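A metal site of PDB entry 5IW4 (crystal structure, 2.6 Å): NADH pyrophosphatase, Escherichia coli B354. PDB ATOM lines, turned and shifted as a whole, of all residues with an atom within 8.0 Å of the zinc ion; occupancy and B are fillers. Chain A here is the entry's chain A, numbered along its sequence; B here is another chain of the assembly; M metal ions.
The zinc ion is bound by the side-chain sulfur (SG) of Cys 120 (2.3 Å), the side-chain sulfur (SG) of Cys 117 (2.3 Å), the side-chain sulfur (SG) of Cys 102 (2.4 Å) and the side-chain sulfur (SG) of Cys 99 (2.4 Å).
The zinc ion has four donor atoms within binding distance.
N of Cys 117 is in hydrogen-bond range of O of Glu 122 (3.1 Å).
N of Glu 122 lies close to SG of Cys 120 (3.7 Å).
N of His 104 lies close to SG of Cys 102, 3.7 Å away.
O of His 104 is in hydrogen-bond range of N of Cys 99.
The side-chain sulfur (SG) of Cys 117 sits close to the backbone NH (N) of His 119 (3.4 Å).
The backbone NH (N) of Tyr 101 sits close to the side-chain sulfur (SG) of Cys 99, 3.4 Å away.
Along chain A the residues within 4 Å of the zinc ion span positions 99 to 120.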
ATOM      1  N   TYR A  98      10.587  11.609  31.793  1.00  0.00           N
ATOM      2  CA  TYR A  98      10.967  11.918  30.425  1.00  0.00           C
ATOM      3  C   TYR A  98      10.225  11.034  29.435  1.00  0.00           C
ATOM      4  O   TYR A  98       9.870   9.898  29.751  1.00  0.00           O
ATOM      5  CB  TYR A  98      12.466  11.737  30.221  1.00  0.00           C
ATOM      6  CG  TYR A  98      13.311  12.684  31.024  1.00  0.00           C
ATOM      7  CD1 TYR A  98      13.674  13.921  30.521  1.00  0.00           C
ATOM      8  CD2 TYR A  98      13.754  12.340  32.303  1.00  0.00           C
ATOM      9  CE1 TYR A  98      14.453  14.792  31.269  1.00  0.00           C
ATOM     10  CE2 TYR A  98      14.522  13.191  33.050  1.00  0.00           C
ATOM     11  CZ  TYR A  98      14.872  14.424  32.529  1.00  0.00           C
ATOM     12  OH  TYR A  98      15.640  15.276  33.277  1.00  0.00           O
ATOM     13  N   CYS A  99      10.006  11.549  28.232  1.00  0.00           N
ATOM     14  CA  CYS A  99       9.360  10.783  27.184  1.00  0.00           C
ATOM     15  C   CYS A  99      10.293   9.732  26.603  1.00  0.00           C
ATOM     16  O   CYS A  99      11.396  10.046  26.155  1.00  0.00           O
ATOM     17  CB  CYS A  99       8.858  11.701  26.076  1.00  0.00           C
ATOM     18  SG  CYS A  99       8.045  10.804  24.742  1.00  0.00           S
ATOM     19  N   GLY A 100       9.841   8.479  26.601  1.00  0.00           N
ATOM     20  CA  GLY A 100      10.637   7.386  26.051  1.00  0.00           C
ATOM     21  C   GLY A 100      10.861   7.504  24.552  1.00  0.00           C
ATOM     22  O   GLY A 100      11.891   7.060  24.034  1.00  0.00           O
ATOM     23  N   TYR A 101       9.907   8.111  23.857  1.00  0.00           N
ATOM     24  CA  TYR A 101       9.990   8.253  22.406  1.00  0.00           C
ATOM     25  C   TYR A 101      11.021   9.295  21.960  1.00  0.00           C
ATOM     26  O   TYR A 101      11.899   8.993  21.145  1.00  0.00           O
ATOM     27  CB  TYR A 101       8.623   8.631  21.827  1.00  0.00           C
ATOM     28  CG  TYR A 101       7.566   7.552  21.887  1.00  0.00           C
ATOM     29  CD1 TYR A 101       7.367   6.698  20.812  1.00  0.00           C
ATOM     30  CD2 TYR A 101       6.754   7.420  23.001  1.00  0.00           C
ATOM     31  CE1 TYR A 101       6.386   5.719  20.846  1.00  0.00           C
ATOM     32  CE2 TYR A 101       5.776   6.439  23.055  1.00  0.00           C
ATOM     33  CZ  TYR A 101       5.594   5.595  21.978  1.00  0.00           C
ATOM     34  OH  TYR A 101       4.622   4.622  22.011  1.00  0.00           O
ATOM     35  N   CYS A 102      10.906  10.514  22.490  1.00  0.00           N
ATOM     36  CA  CYS A 102      11.744  11.610  22.012  1.00  0.00           C
ATOM     37  C   CYS A 102      12.683  12.219  23.076  1.00  0.00           C
ATOM     38  O   CYS A 102      13.515  13.056  22.751  1.00  0.00           O
ATOM     39  CB  CYS A 102      10.885  12.715  21.381  1.00  0.00           C
ATOM     40  SG  CYS A 102      10.022  13.776  22.563  1.00  0.00           S
ATOM     41  N   GLY A 103      12.548  11.800  24.319  1.00  0.00           N
ATOM     42  CA  GLY A 103      13.482  12.223  25.348  1.00  0.00           C
ATOM     43  C   GLY A 103      13.188  13.558  26.001  1.00  0.00           C
ATOM     44  O   GLY A 103      13.914  14.000  26.886  1.00  0.00           O
ATOM     45  N   HIS A 104      12.113  14.219  25.567  1.00  0.00           N
ATOM     46  CA  HIS A 104      11.712  15.471  26.181  1.00  0.00           C
ATOM     47  C   HIS A 104      10.953  15.217  27.479  1.00  0.00           C
ATOM     48  O   HIS A 104      10.539  14.089  27.746  1.00  0.00           O
ATOM     49  CB  HIS A 104      10.875  16.309  25.219  1.00  0.00           C
ATOM     50  CG  HIS A 104      11.651  16.887  24.087  1.00  0.00           C
ATOM     51  ND1 HIS A 104      11.698  18.232  23.803  1.00  0.00           N
ATOM     52  CD2 HIS A 104      12.447  16.297  23.150  1.00  0.00           C
ATOM     53  CE1 HIS A 104      12.462  18.453  22.756  1.00  0.00           C
ATOM     54  NE2 HIS A 104      12.929  17.286  22.340  1.00  0.00           N
ATOM     55  N   GLU A 105      10.786  16.255  28.289  1.00  0.00           N
ATOM     56  CA  GLU A 105      10.097  16.130  29.565  1.00  0.00           C
ATOM     57  C   GLU A 105       8.579  16.041  29.382  1.00  0.00           C
ATOM     58  O   GLU A 105       8.002  16.676  28.509  1.00  0.00           O
ATOM     59  CB  GLU A 105      10.468  17.300  30.482  1.00  0.00           C
ATOM     60  CG  GLU A 105      11.953  17.401  30.743  1.00  0.00           C
ATOM     61  CD  GLU A 105      12.322  18.657  31.514  1.00  0.00           C
ATOM     62  OE1 GLU A 105      11.398  19.354  31.983  1.00  0.00           O
ATOM     63  OE2 GLU A 105      13.531  18.937  31.636  1.00  0.00           O
ATOM     64  N   MET A 106       7.942  15.246  30.236  1.00  0.00           N
ATOM     65  CA  MET A 106       6.494  15.027  30.142  1.00  0.00           C
ATOM     66  C   MET A 106       5.727  15.704  31.275  1.00  0.00           C
ATOM     67  O   MET A 106       6.298  16.112  32.276  1.00  0.00           O
ATOM     68  CB  MET A 106       6.180  13.532  30.105  1.00  0.00           C
ATOM     69  CG  MET A 106       6.537  12.864  28.793  1.00  0.00           C
ATOM     70  SD  MET A 106       5.738  11.256  28.600  1.00  0.00           S
ATOM     71  CE  MET A 106       6.805  10.233  29.587  1.00  0.00           C
ATOM     72  N   LEU A 116       1.652  12.976  29.346  1.00  0.00           N
ATOM     73  CA  LEU A 116       1.642  13.448  27.980  1.00  0.00           C
ATOM     74  C   LEU A 116       2.949  14.175  27.642  1.00  0.00           C
ATOM     75  O   LEU A 116       3.539  14.823  28.507  1.00  0.00           O
ATOM     76  CB  LEU A 116       0.450  14.389  27.753  1.00  0.00           C
ATOM     77  CG  LEU A 116      -0.862  14.062  28.471  1.00  0.00           C
ATOM     78  CD1 LEU A 116      -1.936  15.063  28.065  1.00  0.00           C
ATOM     79  CD2 LEU A 116      -1.328  12.648  28.204  1.00  0.00           C
ATOM     80  N   CYS A 117       3.381  14.053  26.391  1.00  0.00           N
ATOM     81  CA  CYS A 117       4.642  14.670  25.981  1.00  0.00           C
ATOM     82  C   CYS A 117       4.429  16.071  25.442  1.00  0.00           C
ATOM     83  O   CYS A 117       3.551  16.309  24.621  1.00  0.00           O
ATOM     84  CB  CYS A 117       5.354  13.814  24.925  1.00  0.00           C
ATOM     85  SG  CYS A 117       6.967  14.476  24.415  1.00  0.00           S
ATOM     86  N   SER A 118       5.255  17.001  25.911  1.00  0.00           N
ATOM     87  CA  SER A 118       5.197  18.384  25.465  1.00  0.00           C
ATOM     88  C   SER A 118       5.603  18.502  23.995  1.00  0.00           C
ATOM     89  O   SER A 118       4.971  19.226  23.231  1.00  0.00           O
ATOM     90  CB  SER A 118       6.119  19.239  26.318  1.00  0.00           C
ATOM     91  OG  SER A 118       7.375  18.598  26.488  1.00  0.00           O
ATOM     92  N   HIS A 119       6.628  17.762  23.637  1.00  0.00           N
ATOM     93  CA  HIS A 119       7.189  17.875  22.322  1.00  0.00           C
ATOM     94  C   HIS A 119       6.469  17.060  21.293  1.00  0.00           C
ATOM     95  O   HIS A 119       5.965  17.623  20.350  1.00  0.00           O
ATOM     96  CB  HIS A 119       8.665  17.515  22.353  1.00  0.00           C
ATOM     97  CG  HIS A 119       9.370  17.818  21.068  1.00  0.00           C
ATOM     98  ND1 HIS A 119       9.875  19.063  20.785  1.00  0.00           N
ATOM     99  CD2 HIS A 119       9.617  17.049  19.981  1.00  0.00           C
ATOM    100  CE1 HIS A 119      10.399  19.049  19.578  1.00  0.00           C
ATOM    101  NE2 HIS A 119      10.263  17.837  19.074  1.00  0.00           N
ATOM    102  N   CYS A 120       6.432  15.754  21.467  1.00  0.00           N
ATOM    103  CA  CYS A 120       5.776  14.855  20.522  1.00  0.00           C
ATOM    104  C   CYS A 120       4.345  14.525  20.935  1.00  0.00           C
ATOM    105  O   CYS A 120       3.851  15.012  21.952  1.00  0.00           O
ATOM    106  CB  CYS A 120       6.589  13.578  20.300  1.00  0.00           C
ATOM    107  SG  CYS A 120       6.547  12.341  21.632  1.00  0.00           S
ATOM    108  N   ARG A 121       3.694  13.706  20.149  1.00  0.00           N
ATOM    109  CA  ARG A 121       2.298  13.427  20.346  1.00  0.00           C
ATOM    110  C   ARG A 121       2.024  12.138  21.094  1.00  0.00           C
ATOM    111  O   ARG A 121       1.033  11.477  20.871  1.00  0.00           O
ATOM    112  CB  ARG A 121       1.576  13.389  18.985  1.00  0.00           C
ATOM    113  CG  ARG A 121       1.548  14.726  18.265  1.00  0.00           C
ATOM    114  CD  ARG A 121       0.796  14.687  16.939  1.00  0.00           C
ATOM    115  NE  ARG A 121       0.852  15.973  16.251  1.00  0.00           N
ATOM    116  CZ  ARG A 121       0.383  16.184  15.027  1.00  0.00           C
ATOM    117  NH1 ARG A 121      -0.188  15.189  14.354  1.00  0.00           N
ATOM    118  NH2 ARG A 121       0.477  17.383  14.478  1.00  0.00           N
ATOM    119  N   GLU A 122       2.893  11.782  22.009  1.00  0.00           N
ATOM    120  CA  GLU A 122       2.806  10.475  22.640  1.00  0.00           C
ATOM    121  C   GLU A 122       2.322  10.492  24.085  1.00  0.00           C
ATOM    122  O   GLU A 122       2.539  11.458  24.829  1.00  0.00           O
ATOM    123  CB  GLU A 122       4.126   9.715  22.523  1.00  0.00           C
ATOM    124  CG  GLU A 122       4.557   9.463  21.079  1.00  0.00           C
ATOM    125  CD  GLU A 122       3.688   8.438  20.355  1.00  0.00           C
ATOM    126  OE1 GLU A 122       2.736   7.901  20.961  1.00  0.00           O
ATOM    127  OE2 GLU A 122       3.963   8.183  19.163  1.00  0.00           O
ATOM    128  N   ARG A 123       1.661   9.424  24.492  1.00  0.00           N
ATOM    129  CA  ARG A 123       1.075   9.274  25.799  1.00  0.00           C
ATOM    130  C   ARG A 123       1.559   8.000  26.482  1.00  0.00           C
ATOM    131  O   ARG A 123       2.028   7.103  25.844  1.00  0.00           O
ATOM    132  CB  ARG A 123      -0.446   9.183  25.678  1.00  0.00           C
ATOM    133  CG  ARG A 123      -1.133  10.417  25.170  1.00  0.00           C
ATOM    134  CD  ARG A 123      -2.614  10.213  25.083  1.00  0.00           C
ATOM    135  NE  ARG A 123      -3.404  11.376  25.475  1.00  0.00           N
ATOM    136  CZ  ARG A 123      -4.059  12.159  24.638  1.00  0.00           C
ATOM    137  NH1 ARG A 123      -4.762  13.177  25.074  1.00  0.00           N
ATOM    138  NH2 ARG A 123      -4.002  11.923  23.334  1.00  0.00           N
ATOM    139  N   TYR A 124       1.430   7.939  27.795  1.00  0.00           N
ATOM    140  CA  TYR A 124       1.659   6.722  28.540  1.00  0.00           C
ATOM    141  C   TYR A 124       0.564   6.586  29.572  1.00  0.00           C
ATOM    142  O   TYR A 124       0.074   7.587  30.100  1.00  0.00           O
ATOM    143  CB  TYR A 124       3.006   6.736  29.247  1.00  0.00           C
ATOM    144  CG  TYR A 124       4.216   6.680  28.341  1.00  0.00           C
ATOM    145  CD1 TYR A 124       4.719   5.469  27.895  1.00  0.00           C
ATOM    146  CD2 TYR A 124       4.851   7.849  27.947  1.00  0.00           C
ATOM    147  CE1 TYR A 124       5.837   5.425  27.068  1.00  0.00           C
ATOM    148  CE2 TYR A 124       5.965   7.812  27.131  1.00  0.00           C
ATOM    149  CZ  TYR A 124       6.454   6.604  26.688  1.00  0.00           C
ATOM    150  OH  TYR A 124       7.558   6.563  25.864  1.00  0.00           O
ATOM    151  N   TYR B  98      14.500   6.396  24.875  1.00  0.00           N
ATOM    152  CA  TYR B  98      15.047   7.079  26.036  1.00  0.00           C
ATOM    153  C   TYR B  98      14.386   6.534  27.303  1.00  0.00           C
ATOM    154  O   TYR B  98      13.301   5.961  27.247  1.00  0.00           O
ATOM    155  CB  TYR B  98      14.820   8.589  25.937  1.00  0.00           C
ATOM    156  CG  TYR B  98      15.373   9.231  24.688  1.00  0.00           C
ATOM    157  CD1 TYR B  98      16.652   9.784  24.667  1.00  0.00           C
ATOM    158  CD2 TYR B  98      14.614   9.310  23.526  1.00  0.00           C
ATOM    159  CE1 TYR B  98      17.164  10.380  23.523  1.00  0.00           C
ATOM    160  CE2 TYR B  98      15.110   9.910  22.376  1.00  0.00           C
ATOM    161  CZ  TYR B  98      16.383  10.442  22.384  1.00  0.00           C
ATOM    162  OH  TYR B  98      16.873  11.035  21.244  1.00  0.00           O
HETATM  163 ZN    ZN M   1       8.008  12.739  23.298  1.00  0.00          ZN
